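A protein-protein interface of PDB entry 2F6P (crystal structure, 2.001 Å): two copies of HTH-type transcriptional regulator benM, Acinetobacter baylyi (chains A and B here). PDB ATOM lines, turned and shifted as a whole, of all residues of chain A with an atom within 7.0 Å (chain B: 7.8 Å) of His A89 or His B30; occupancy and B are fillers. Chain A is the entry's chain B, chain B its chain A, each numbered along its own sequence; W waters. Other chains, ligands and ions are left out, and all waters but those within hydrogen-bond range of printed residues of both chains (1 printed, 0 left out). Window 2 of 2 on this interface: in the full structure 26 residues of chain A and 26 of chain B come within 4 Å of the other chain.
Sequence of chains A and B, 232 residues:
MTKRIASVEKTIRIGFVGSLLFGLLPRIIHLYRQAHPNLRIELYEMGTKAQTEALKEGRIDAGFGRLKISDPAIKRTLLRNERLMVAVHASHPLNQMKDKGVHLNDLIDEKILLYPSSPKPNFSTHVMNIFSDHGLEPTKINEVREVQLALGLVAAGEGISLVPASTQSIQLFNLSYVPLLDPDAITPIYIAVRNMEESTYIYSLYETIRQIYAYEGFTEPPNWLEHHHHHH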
ATOM      1  N   ALA A  87     -23.048  31.939  -0.519  1.00  0.00           N
ATOM      2  CA  ALA A  87     -22.869  30.498  -0.630  1.00  0.00           C
ATOM      3  C   ALA A  87     -24.243  29.839  -0.697  1.00  0.00           C
ATOM      4  O   ALA A  87     -25.056  30.001   0.216  1.00  0.00           O
ATOM      5  CB  ALA A  87     -22.098  29.972   0.554  1.00  0.00           C
ATOM      6  N   VAL A  88     -24.485  29.094  -1.771  1.00  0.00           N
ATOM      7  CA  VAL A  88     -25.759  28.417  -1.993  1.00  0.00           C
ATOM      8  C   VAL A  88     -25.523  26.981  -2.448  1.00  0.00           C
ATOM      9  O   VAL A  88     -24.442  26.647  -2.937  1.00  0.00           O
ATOM     10  CB  VAL A  88     -26.617  29.147  -3.061  1.00  0.00           C
ATOM     11  CG1 VAL A  88     -26.822  30.602  -2.683  1.00  0.00           C
ATOM     12  CG2 VAL A  88     -25.989  29.041  -4.460  1.00  0.00           C
ATOM     13  N   HIS A  89     -26.547  26.138  -2.296  1.00  0.00           N
ATOM     14  CA  HIS A  89     -26.536  24.815  -2.908  1.00  0.00           C
ATOM     15  C   HIS A  89     -26.726  24.981  -4.416  1.00  0.00           C
ATOM     16  O   HIS A  89     -27.514  25.817  -4.856  1.00  0.00           O
ATOM     17  CB  HIS A  89     -27.634  23.922  -2.322  1.00  0.00           C
ATOM     18  CG  HIS A  89     -27.551  22.498  -2.772  1.00  0.00           C
ATOM     19  ND1 HIS A  89     -28.187  22.042  -3.903  1.00  0.00           N
ATOM     20  CD2 HIS A  89     -26.895  21.433  -2.255  1.00  0.00           C
ATOM     21  CE1 HIS A  89     -27.933  20.755  -4.064  1.00  0.00           C
ATOM     22  NE2 HIS A  89     -27.148  20.363  -3.076  1.00  0.00           N
ATOM     23  N   ALA A  90     -26.011  24.181  -5.200  1.00  0.00           N
ATOM     24  CA  ALA A  90     -25.977  24.337  -6.661  1.00  0.00           C
ATOM     25  C   ALA A  90     -27.354  24.259  -7.344  1.00  0.00           C
ATOM     26  O   ALA A  90     -27.527  24.792  -8.435  1.00  0.00           O
ATOM     27  CB  ALA A  90     -25.038  23.311  -7.269  1.00  0.00           C
ATOM     28  N   SER A  91     -28.310  23.589  -6.701  1.00  0.00           N
ATOM     29  CA  SER A  91     -29.691  23.477  -7.194  1.00  0.00           C
ATOM     30  C   SER A  91     -30.615  24.614  -6.736  1.00  0.00           C
ATOM     31  O   SER A  91     -31.784  24.646  -7.128  1.00  0.00           O
ATOM     32  CB  SER A  91     -30.306  22.145  -6.748  1.00  0.00           C
ATOM     33  OG  SER A  91     -30.757  22.222  -5.402  1.00  0.00           O
ATOM     34  N   HIS A  92     -30.111  25.527  -5.906  1.00  0.00           N
ATOM     35  CA  HIS A  92     -30.883  26.705  -5.498  1.00  0.00           C
ATOM     36  C   HIS A  92     -31.119  27.618  -6.706  1.00  0.00           C
ATOM     37  O   HIS A  92     -30.201  27.813  -7.519  1.00  0.00           O
ATOM     38  CB  HIS A  92     -30.154  27.490  -4.403  1.00  0.00           C
ATOM     39  CG  HIS A  92     -31.064  28.308  -3.540  1.00  0.00           C
ATOM     40  ND1 HIS A  92     -31.480  29.576  -3.881  1.00  0.00           N
ATOM     41  CD2 HIS A  92     -31.649  28.030  -2.350  1.00  0.00           C
ATOM     42  CE1 HIS A  92     -32.274  30.048  -2.938  1.00  0.00           C
ATOM     43  NE2 HIS A  92     -32.395  29.128  -1.998  1.00  0.00           N
ATOM     44  N   PRO A  93     -32.347  28.172  -6.841  1.00  0.00           N
ATOM     45  CA  PRO A  93     -32.661  29.121  -7.915  1.00  0.00           C
ATOM     46  C   PRO A  93     -31.682  30.293  -8.074  1.00  0.00           C
ATOM     47  O   PRO A  93     -31.455  30.752  -9.189  1.00  0.00           O
ATOM     48  CB  PRO A  93     -34.044  29.646  -7.517  1.00  0.00           C
ATOM     49  CG  PRO A  93     -34.659  28.535  -6.764  1.00  0.00           C
ATOM     50  CD  PRO A  93     -33.531  27.904  -5.998  1.00  0.00           C
ATOM     51  N   LEU A  94     -31.126  30.777  -6.965  1.00  0.00           N
ATOM     52  CA  LEU A  94     -30.118  31.847  -6.984  1.00  0.00           C
ATOM     53  C   LEU A  94     -28.861  31.456  -7.750  1.00  0.00           C
ATOM     54  O   LEU A  94     -28.175  32.319  -8.300  1.00  0.00           O
ATOM     55  CB  LEU A  94     -29.723  32.256  -5.562  1.00  0.00           C
ATOM     56  CG  LEU A  94     -30.761  33.020  -4.736  1.00  0.00           C
ATOM     57  CD1 LEU A  94     -30.318  33.121  -3.283  1.00  0.00           C
ATOM     58  CD2 LEU A  94     -31.014  34.403  -5.318  1.00  0.00           C
ATOM     59  N   ASN A  95     -28.554  30.160  -7.785  1.00  0.00           N
ATOM     60  CA  ASN A  95     -27.388  29.681  -8.524  1.00  0.00           C
ATOM     61  C   ASN A  95     -27.493  29.898 -10.033  1.00  0.00           C
ATOM     62  O   ASN A  95     -26.485  29.851 -10.733  1.00  0.00           O
ATOM     63  CB  ASN A  95     -27.099  28.203  -8.237  1.00  0.00           C
ATOM     64  CG  ASN A  95     -25.665  27.817  -8.576  1.00  0.00           C
ATOM     65  OD1 ASN A  95     -25.397  26.735  -9.092  1.00  0.00           O
ATOM     66  ND2 ASN A  95     -24.739  28.715  -8.295  1.00  0.00           N
ATOM     67  N   LEU A 153     -23.397  23.038   6.109  1.00  0.00           N
ATOM     68  CA  LEU A 153     -24.860  23.095   6.242  1.00  0.00           C
ATOM     69  C   LEU A 153     -25.539  23.543   4.938  1.00  0.00           C
ATOM     70  O   LEU A 153     -26.558  22.974   4.540  1.00  0.00           O
ATOM     71  CB  LEU A 153     -25.252  24.028   7.398  1.00  0.00           C
ATOM     72  CG  LEU A 153     -25.420  23.448   8.812  1.00  0.00           C
ATOM     73  CD1 LEU A 153     -24.484  22.287   9.097  1.00  0.00           C
ATOM     74  CD2 LEU A 153     -25.248  24.543   9.856  1.00  0.00           C
ATOM     75  N   VAL A 154     -24.977  24.558   4.280  1.00  0.00           N
ATOM     76  CA  VAL A 154     -25.456  24.992   2.960  1.00  0.00           C
ATOM     77  C   VAL A 154     -25.434  23.826   1.967  1.00  0.00           C
ATOM     78  O   VAL A 154     -26.412  23.597   1.255  1.00  0.00           O
ATOM     79  CB  VAL A 154     -24.611  26.180   2.391  1.00  0.00           C
ATOM     80  CG1 VAL A 154     -24.920  26.431   0.909  1.00  0.00           C
ATOM     81  CG2 VAL A 154     -24.845  27.451   3.202  1.00  0.00           C
ATOM     82  N   ALA A 155     -24.314  23.105   1.922  1.00  0.00           N
ATOM     83  CA  ALA A 155     -24.159  21.949   1.033  1.00  0.00           C
ATOM     84  C   ALA A 155     -25.096  20.790   1.393  1.00  0.00           C
ATOM     85  O   ALA A 155     -25.435  19.983   0.532  1.00  0.00           O
ATOM     86  CB  ALA A 155     -22.717  21.462   1.037  1.00  0.00           C
ATOM     87  N   ALA A 156     -25.483  20.702   2.664  1.00  0.00           N
ATOM     88  CA  ALA A 156     -26.455  19.709   3.120  1.00  0.00           C
ATOM     89  C   ALA A 156     -27.910  20.136   2.883  1.00  0.00           C
ATOM     90  O   ALA A 156     -28.827  19.344   3.111  1.00  0.00           O
ATOM     91  CB  ALA A 156     -26.237  19.396   4.600  1.00  0.00           C
ATOM     92  N   GLY A 157     -28.123  21.379   2.449  1.00  0.00           N
ATOM     93  CA  GLY A 157     -29.464  21.883   2.132  1.00  0.00           C
ATOM     94  C   GLY A 157     -30.125  22.725   3.217  1.00  0.00           C
ATOM     95  O   GLY A 157     -31.343  22.892   3.212  1.00  0.00           O
ATOM     96  N   GLU A 158     -29.331  23.277   4.133  1.00  0.00           N
ATOM     97  CA  GLU A 158     -29.872  23.996   5.296  1.00  0.00           C
ATOM     98  C   GLU A 158     -30.198  25.468   5.031  1.00  0.00           C
ATOM     99  O   GLU A 158     -30.894  26.094   5.829  1.00  0.00           O
ATOM    100  CB  GLU A 158     -28.917  23.887   6.493  1.00  0.00           C
ATOM    101  CG  GLU A 158     -28.834  22.472   7.101  1.00  0.00           C
ATOM    102  CD  GLU A 158     -29.867  22.221   8.196  1.00  0.00           C
ATOM    103  OE1 GLU A 158     -29.936  23.024   9.148  1.00  0.00           O
ATOM    104  OE2 GLU A 158     -30.601  21.211   8.117  1.00  0.00           O
ATOM    105  N   GLY A 159     -29.708  26.023   3.926  1.00  0.00           N
ATOM    106  CA  GLY A 159     -30.010  27.411   3.568  1.00  0.00           C
ATOM    107  C   GLY A 159     -28.911  28.042   2.739  1.00  0.00           C
ATOM    108  O   GLY A 159     -28.279  27.361   1.935  1.00  0.00           O
ATOM    109  N   ILE A 160     -28.712  29.349   2.922  1.00  0.00           N
ATOM    110  CA  ILE A 160     -27.619  30.100   2.282  1.00  0.00           C
ATOM    111  C   ILE A 160     -26.803  30.814   3.366  1.00  0.00           C
ATOM    112  O   ILE A 160     -27.233  30.892   4.520  1.00  0.00           O
ATOM    113  CB  ILE A 160     -28.150  31.146   1.261  1.00  0.00           C
ATOM    114  CG1 ILE A 160     -28.898  32.281   1.970  1.00  0.00           C
ATOM    115  CG2 ILE A 160     -29.057  30.478   0.217  1.00  0.00           C
ATOM    116  CD1 ILE A 160     -29.342  33.402   1.052  1.00  0.00           C
ATOM    117  N   PHE A 173     -18.741  19.602  -2.767  1.00  0.00           N
ATOM    118  CA  PHE A 173     -19.620  19.123  -3.821  1.00  0.00           C
ATOM    119  C   PHE A 173     -20.985  19.790  -3.698  1.00  0.00           C
ATOM    120  O   PHE A 173     -21.588  19.792  -2.622  1.00  0.00           O
ATOM    121  CB  PHE A 173     -19.767  17.605  -3.758  1.00  0.00           C
ATOM    122  CG  PHE A 173     -20.714  17.050  -4.777  1.00  0.00           C
ATOM    123  CD1 PHE A 173     -20.336  16.948  -6.108  1.00  0.00           C
ATOM    124  CD2 PHE A 173     -21.981  16.625  -4.409  1.00  0.00           C
ATOM    125  CE1 PHE A 173     -21.205  16.434  -7.056  1.00  0.00           C
ATOM    126  CE2 PHE A 173     -22.855  16.106  -5.356  1.00  0.00           C
ATOM    127  CZ  PHE A 173     -22.464  16.013  -6.680  1.00  0.00           C
ATOM    128  N   ASN A 174     -21.442  20.373  -4.808  1.00  0.00           N
ATOM    129  CA  ASN A 174     -22.720  21.091  -4.892  1.00  0.00           C
ATOM    130  C   ASN A 174     -22.832  22.347  -4.023  1.00  0.00           C
ATOM    131  O   ASN A 174     -23.934  22.824  -3.760  1.00  0.00           O
ATOM    132  CB  ASN A 174     -23.907  20.142  -4.645  1.00  0.00           C
ATOM    133  CG  ASN A 174     -24.363  19.427  -5.903  1.00  0.00           C
ATOM    134  OD1 ASN A 174     -23.898  19.707  -7.010  1.00  0.00           O
ATOM    135  ND2 ASN A 174     -25.290  18.499  -5.735  1.00  0.00           N
ATOM    136  N   LEU A 175     -21.691  22.888  -3.597  1.00  0.00           N
ATOM    137  CA  LEU A 175     -21.641  24.210  -2.987  1.00  0.00           C
ATOM    138  C   LEU A 175     -21.192  25.200  -4.051  1.00  0.00           C
ATOM    139  O   LEU A 175     -20.174  24.980  -4.722  1.00  0.00           O
ATOM    140  CB  LEU A 175     -20.660  24.236  -1.813  1.00  0.00           C
ATOM    141  CG  LEU A 175     -20.402  25.593  -1.146  1.00  0.00           C
ATOM    142  CD1 LEU A 175     -21.645  26.100  -0.434  1.00  0.00           C
ATOM    143  CD2 LEU A 175     -19.222  25.499  -0.175  1.00  0.00           C
ATOM    144  N   SER A 176     -21.936  26.295  -4.187  1.00  0.00           N
ATOM    145  CA  SER A 176     -21.623  27.326  -5.173  1.00  0.00           C
ATOM    146  C   SER A 176     -21.552  28.702  -4.518  1.00  0.00           C
ATOM    147  O   SER A 176     -22.332  29.005  -3.610  1.00  0.00           O
ATOM    148  CB  SER A 176     -22.677  27.330  -6.279  1.00  0.00           C
ATOM    149  OG  SER A 176     -22.314  28.231  -7.309  1.00  0.00           O
ATOM    150  N   LEU B  24     -18.456  13.180   2.032  1.00  0.00           N
ATOM    151  CA  LEU B  24     -19.722  12.812   1.385  1.00  0.00           C
ATOM    152  C   LEU B  24     -20.980  13.088   2.218  1.00  0.00           C
ATOM    153  O   LEU B  24     -22.093  12.979   1.702  1.00  0.00           O
ATOM    154  CB  LEU B  24     -19.701  11.329   0.997  1.00  0.00           C
ATOM    155  CG  LEU B  24     -18.586  10.870   0.048  1.00  0.00           C
ATOM    156  CD1 LEU B  24     -18.516   9.351  -0.020  1.00  0.00           C
ATOM    157  CD2 LEU B  24     -18.778  11.449  -1.335  1.00  0.00           C
ATOM    158  N   LEU B  25     -20.825  13.443   3.490  1.00  0.00           N
ATOM    159  CA  LEU B  25     -21.994  13.548   4.380  1.00  0.00           C
ATOM    160  C   LEU B  25     -23.034  14.579   3.916  1.00  0.00           C
ATOM    161  O   LEU B  25     -24.230  14.264   3.901  1.00  0.00           O
ATOM    162  CB  LEU B  25     -21.571  13.790   5.836  1.00  0.00           C
ATOM    163  CG  LEU B  25     -22.686  13.883   6.884  1.00  0.00           C
ATOM    164  CD1 LEU B  25     -23.556  12.643   6.880  1.00  0.00           C
ATOM    165  CD2 LEU B  25     -22.081  14.117   8.270  1.00  0.00           C
ATOM    166  N   PRO B  26     -22.596  15.801   3.542  1.00  0.00           N
ATOM    167  CA  PRO B  26     -23.544  16.794   3.032  1.00  0.00           C
ATOM    168  C   PRO B  26     -24.421  16.335   1.862  1.00  0.00           C
ATOM    169  O   PRO B  26     -25.626  16.567   1.898  1.00  0.00           O
ATOM    170  CB  PRO B  26     -22.642  17.965   2.623  1.00  0.00           C
ATOM    171  CG  PRO B  26     -21.462  17.838   3.516  1.00  0.00           C
ATOM    172  CD  PRO B  26     -21.230  16.359   3.612  1.00  0.00           C
ATOM    173  N   ARG B  27     -23.844  15.691   0.843  1.00  0.00           N
ATOM    174  CA  ARG B  27     -24.633  15.217  -0.298  1.00  0.00           C
ATOM    175  C   ARG B  27     -25.536  14.039   0.104  1.00  0.00           C
ATOM    176  O   ARG B  27     -26.604  13.848  -0.473  1.00  0.00           O
ATOM    177  CB  ARG B  27     -23.738  14.892  -1.511  1.00  0.00           C
ATOM    178  CG  ARG B  27     -23.016  13.549  -1.498  1.00  0.00           C
ATOM    179  CD  ARG B  27     -22.010  13.447  -2.657  1.00  0.00           C
ATOM    180  NE  ARG B  27     -20.697  14.003  -2.315  1.00  0.00           N
ATOM    181  CZ  ARG B  27     -19.713  14.236  -3.184  1.00  0.00           C
ATOM    182  NH1 ARG B  27     -19.862  13.965  -4.479  1.00  0.00           N
ATOM    183  NH2 ARG B  27     -18.563  14.746  -2.755  1.00  0.00           N
ATOM    184  N   ILE B  28     -25.113  13.267   1.107  1.00  0.00           N
ATOM    185  CA  ILE B  28     -25.970  12.213   1.687  1.00  0.00           C
ATOM    186  C   ILE B  28     -27.200  12.833   2.361  1.00  0.00           C
ATOM    187  O   ILE B  28     -28.347  12.444   2.082  1.00  0.00           O
ATOM    188  CB  ILE B  28     -25.179  11.309   2.683  1.00  0.00           C
ATOM    189  CG1 ILE B  28     -24.196  10.421   1.921  1.00  0.00           C
ATOM    190  CG2 ILE B  28     -26.122  10.425   3.498  1.00  0.00           C
ATOM    191  CD1 ILE B  28     -23.111   9.800   2.781  1.00  0.00           C
ATOM    192  N   ILE B  29     -26.962  13.807   3.239  1.00  0.00           N
ATOM    193  CA  ILE B  29     -28.042  14.522   3.927  1.00  0.00           C
ATOM    194  C   ILE B  29     -28.974  15.237   2.938  1.00  0.00           C
ATOM    195  O   ILE B  29     -30.192  15.247   3.124  1.00  0.00           O
ATOM    196  CB  ILE B  29     -27.477  15.532   4.957  1.00  0.00           C
ATOM    197  CG1 ILE B  29     -26.827  14.774   6.120  1.00  0.00           C
ATOM    198  CG2 ILE B  29     -28.581  16.464   5.480  1.00  0.00           C
ATOM    199  CD1 ILE B  29     -25.957  15.631   7.025  1.00  0.00           C
ATOM    200  N   HIS B  30     -28.410  15.823   1.886  1.00  0.00           N
ATOM    201  CA  HIS B  30     -29.221  16.516   0.892  1.00  0.00           C
ATOM    202  C   HIS B  30     -30.136  15.567   0.107  1.00  0.00           C
ATOM    203  O   HIS B  30     -31.304  15.886  -0.132  1.00  0.00           O
ATOM    204  CB  HIS B  30     -28.359  17.319  -0.082  1.00  0.00           C
ATOM    205  CG  HIS B  30     -29.158  18.245  -0.945  1.00  0.00           C
ATOM    206  ND1 HIS B  30     -29.375  19.565  -0.615  1.00  0.00           N
ATOM    207  CD2 HIS B  30     -29.828  18.030  -2.101  1.00  0.00           C
ATOM    208  CE1 HIS B  30     -30.130  20.129  -1.542  1.00  0.00           C
ATOM    209  NE2 HIS B  30     -30.418  19.218  -2.454  1.00  0.00           N
ATOM    210  N   LEU B  31     -29.603  14.422  -0.307  1.00  0.00           N
ATOM    211  CA  LEU B  31     -30.404  13.421  -1.022  1.00  0.00           C
ATOM    212  C   LEU B  31     -31.480  12.824  -0.111  1.00  0.00           C
ATOM    213  O   LEU B  31     -32.606  12.573  -0.549  1.00  0.00           O
ATOM    214  CB  LEU B  31     -29.512  12.309  -1.573  1.00  0.00           C
ATOM    215  CG  LEU B  31     -30.176  11.291  -2.505  1.00  0.00           C
ATOM    216  CD1 LEU B  31     -30.778  11.982  -3.721  1.00  0.00           C
ATOM    217  CD2 LEU B  31     -29.184  10.219  -2.942  1.00  0.00           C
ATOM    218  N   TYR B  32     -31.122  12.591   1.149  1.00  0.00           N
ATOM    219  CA  TYR B  32     -32.070  12.119   2.159  1.00  0.00           C
ATOM    220  C   TYR B  32     -33.207  13.134   2.359  1.00  0.00           C
ATOM    221  O   TYR B  32     -34.384  12.773   2.343  1.00  0.00           O
ATOM    222  CB  TYR B  32     -31.336  11.854   3.481  1.00  0.00           C
ATOM    223  CG  TYR B  32     -32.212  11.299   4.590  1.00  0.00           C
ATOM    224  CD1 TYR B  32     -32.708  10.001   4.530  1.00  0.00           C
ATOM    225  CD2 TYR B  32     -32.525  12.068   5.705  1.00  0.00           C
ATOM    226  CE1 TYR B  32     -33.505   9.484   5.548  1.00  0.00           C
ATOM    227  CE2 TYR B  32     -33.321  11.559   6.730  1.00  0.00           C
ATOM    228  CZ  TYR B  32     -33.807  10.268   6.643  1.00  0.00           C
ATOM    229  OH  TYR B  32     -34.594   9.761   7.645  1.00  0.00           O
ATOM    230  N   ARG B  33     -32.836  14.402   2.528  1.00  0.00           N
ATOM    231  CA  ARG B  33     -33.790  15.503   2.699  1.00  0.00           C
ATOM    232  C   ARG B  33     -34.809  15.579   1.564  1.00  0.00           C
ATOM    233  O   ARG B  33     -36.002  15.744   1.812  1.00  0.00           O
ATOM    234  CB  ARG B  33     -33.033  16.837   2.794  1.00  0.00           C
ATOM    235  CG  ARG B  33     -33.889  18.043   3.148  1.00  0.00           C
ATOM    236  CD  ARG B  33     -33.102  19.349   3.010  1.00  0.00           C
ATOM    237  NE  ARG B  33     -31.862  19.330   3.790  1.00  0.00           N
ATOM    238  CZ  ARG B  33     -31.763  19.626   5.087  1.00  0.00           C
ATOM    239  NH1 ARG B  33     -32.829  19.973   5.805  1.00  0.00           N
ATOM    240  NH2 ARG B  33     -30.575  19.571   5.680  1.00  0.00           N
ATOM    241  N   GLN B  34     -34.335  15.461   0.325  1.00  0.00           N
ATOM    242  CA  GLN B  34     -35.206  15.561  -0.850  1.00  0.00           C
ATOM    243  C   GLN B  34     -36.204  14.405  -0.956  1.00  0.00           C
ATOM    244  O   GLN B  34     -37.273  14.559  -1.548  1.00  0.00           O
ATOM    245  CB  GLN B  34     -34.375  15.646  -2.137  1.00  0.00           C
ATOM    246  CG  GLN B  34     -33.524  16.909  -2.247  1.00  0.00           C
ATOM    247  CD  GLN B  34     -34.353  18.175  -2.397  1.00  0.00           C
ATOM    248  OE1 GLN B  34     -35.058  18.354  -3.390  1.00  0.00           O
ATOM    249  NE2 GLN B  34     -34.266  19.063  -1.408  1.00  0.00           N
ATOM    250  N   ALA B  35     -35.852  13.256  -0.381  1.00  0.00           N
ATOM    251  CA  ALA B  35     -36.715  12.078  -0.393  1.00  0.00           C
ATOM    252  C   ALA B  35     -37.747  12.094   0.734  1.00  0.00           C
ATOM    253  O   ALA B  35     -38.593  11.202   0.808  1.00  0.00           O
ATOM    254  CB  ALA B  35     -35.874  10.816  -0.298  1.00  0.00           C
ATOM    255  N   HIS B  36     -37.674  13.091   1.617  1.00  0.00           N
ATOM    256  CA  HIS B  36     -38.562  13.158   2.773  1.00  0.00           C
ATOM    257  C   HIS B  36     -39.040  14.582   3.020  1.00  0.00           C
ATOM    258  O   HIS B  36     -38.684  15.191   4.028  1.00  0.00           O
ATOM    259  CB  HIS B  36     -37.846  12.599   4.002  1.00  0.00           C
ATOM    260  CG  HIS B  36     -37.522  11.146   3.883  1.00  0.00           C
ATOM    261  ND1 HIS B  36     -38.407  10.157   4.248  1.00  0.00           N
ATOM    262  CD2 HIS B  36     -36.424  10.513   3.412  1.00  0.00           C
ATOM    263  CE1 HIS B  36     -37.862   8.975   4.020  1.00  0.00           C
ATOM    264  NE2 HIS B  36     -36.658   9.165   3.513  1.00  0.00           N
ATOM    265  N   ILE B  41     -35.311  17.843   9.373  1.00  0.00           N
ATOM    266  CA  ILE B  41     -33.951  17.376   9.639  1.00  0.00           C
ATOM    267  C   ILE B  41     -33.248  18.370  10.547  1.00  0.00           C
ATOM    268  O   ILE B  41     -33.079  19.535  10.180  1.00  0.00           O
ATOM    269  CB  ILE B  41     -33.117  17.244   8.339  1.00  0.00           C
ATOM    270  CG1 ILE B  41     -33.901  16.497   7.255  1.00  0.00           C
ATOM    271  CG2 ILE B  41     -31.775  16.563   8.627  1.00  0.00           C
ATOM    272  CD1 ILE B  41     -34.414  15.146   7.669  1.00  0.00           C
ATOM    273  N   LEU B  43     -29.669  18.993  12.426  1.00  0.00           N
ATOM    274  CA  LEU B  43     -28.280  18.571  12.378  1.00  0.00           C
ATOM    275  C   LEU B  43     -27.533  19.187  13.549  1.00  0.00           C
ATOM    276  O   LEU B  43     -27.634  20.393  13.784  1.00  0.00           O
ATOM    277  CB  LEU B  43     -27.646  19.010  11.061  1.00  0.00           C
ATOM    278  CG  LEU B  43     -28.324  18.482   9.797  1.00  0.00           C
ATOM    279  CD1 LEU B  43     -27.688  19.108   8.564  1.00  0.00           C
ATOM    280  CD2 LEU B  43     -28.245  16.969   9.737  1.00  0.00           C
ATOM    281  N   THR B 208     -29.794   5.654   1.563  1.00  0.00           N
ATOM    282  CA  THR B 208     -29.184   6.829   0.942  1.00  0.00           C
ATOM    283  C   THR B 208     -27.657   6.745   0.934  1.00  0.00           C
ATOM    284  O   THR B 208     -27.020   7.101  -0.063  1.00  0.00           O
ATOM    285  CB  THR B 208     -29.637   8.114   1.654  1.00  0.00           C
ATOM    286  OG1 THR B 208     -31.071   8.145   1.681  1.00  0.00           O
ATOM    287  CG2 THR B 208     -29.104   9.347   0.937  1.00  0.00           C
ATOM    288  N   ILE B 212     -25.228   6.566  -2.632  1.00  0.00           N
ATOM    289  CA  ILE B 212     -24.111   7.471  -2.886  1.00  0.00           C
ATOM    290  C   ILE B 212     -22.789   6.710  -2.942  1.00  0.00           C
ATOM    291  O   ILE B 212     -21.961   6.987  -3.807  1.00  0.00           O
ATOM    292  CB  ILE B 212     -24.096   8.627  -1.858  1.00  0.00           C
ATOM    293  CG1 ILE B 212     -25.265   9.566  -2.170  1.00  0.00           C
ATOM    294  CG2 ILE B 212     -22.776   9.413  -1.907  1.00  0.00           C
ATOM    295  CD1 ILE B 212     -25.754  10.317  -1.020  1.00  0.00           C
HETATM  296  O   HOH W   1     -30.312  21.826  11.637  1.00  0.00           O
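The guanidinium group (NH2) of Arg B33 lies within salt-bridge range of the side-chain carboxylate (OE2) of Glu A158.
A ring nitrogen (ND1) of His B30 sits close to a ring nitrogen (NE2) of His A89, 3.4 Å away.
NE of Arg B33 sits at hydrogen-bond distance from O of Ala A156, 3.1 Å away.
A ring nitrogen (ND1) of His A89 sits at hydrogen-bond distance from the side-chain hydroxyl of Ser A91 (3.0 Å).
The backbone carbonyl oxygen of Leu A153 sits at hydrogen-bond distance from the backbone NH of Glu A158, 2.8 Å away.
O of Ala A155 touches O of Pro B26, 3.7 Å away.
Ala A156 touches Pro B26.
CG2 of Ile B29 touches O of Ala A156 (3.7 Å).
Ala A156 touches His B30 (O to CA, 3.6 Å).
Gly A157 touches His B30.
Gly A157 touches Arg B33.
Ile B41 touches Glu A158 (O to OE2, 3.6 Å).
Glu A158 touches Leu B43.
Phe A173 touches Arg B27.
His A89 touches just one residue of chain B: His B30 (3.3 Å).
Of the printed residues of chain A, His B30 touches His A89, Ala A156 and Gly A157.
No residue of chain B comes within 4 Å of Ala A90.
Of the printed residues of chain B, Gly A157 touches His B30 (3.6 Å) and Arg B33 (3.6 Å).
Of the printed residues of chain A, Pro B26 touches Ala A155 (3.7 Å) and Ala A156 (3.5 Å).
Of the printed residues of chain A, Leu B43 touches Glu A158.
Printed residues of chain B within 4 Å of Ala A156: Pro B26, Ile B29, His B30 and Arg B33.
Printed residues of chain B within 4 Å of Ala A155: Pro B26.
The nearest printed residue of chain B that does not touch His A89 is Arg B27 (6.4 Å).
The nearest printed residue of chain A that does not touch His B30 is Ala A155 (4.003 Å).
Printed residues of chain B that touch a printed residue of chain A: Pro B26, Arg B27, Ile B29, His B30, Arg B33, Ile B41 and Leu B43.
Of the 21 printed residues of chain A, 6 touch a printed residue of chain B.
Hydrophobic or aromatic side chains of chain A within 4 Å of the printed part of chain B: His A89, Ala A155, Ala A156 and Phe A173.
No position is printed for both chains.
Of the 12 pairs that touch across the chains among the printed residues, none has its exchanged pair printed and touching as well.
Water W1 lies within hydrogen-bond range of OE1 of Glu A158 (2.8 Å) and N of Leu B43 (3.0 Å).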
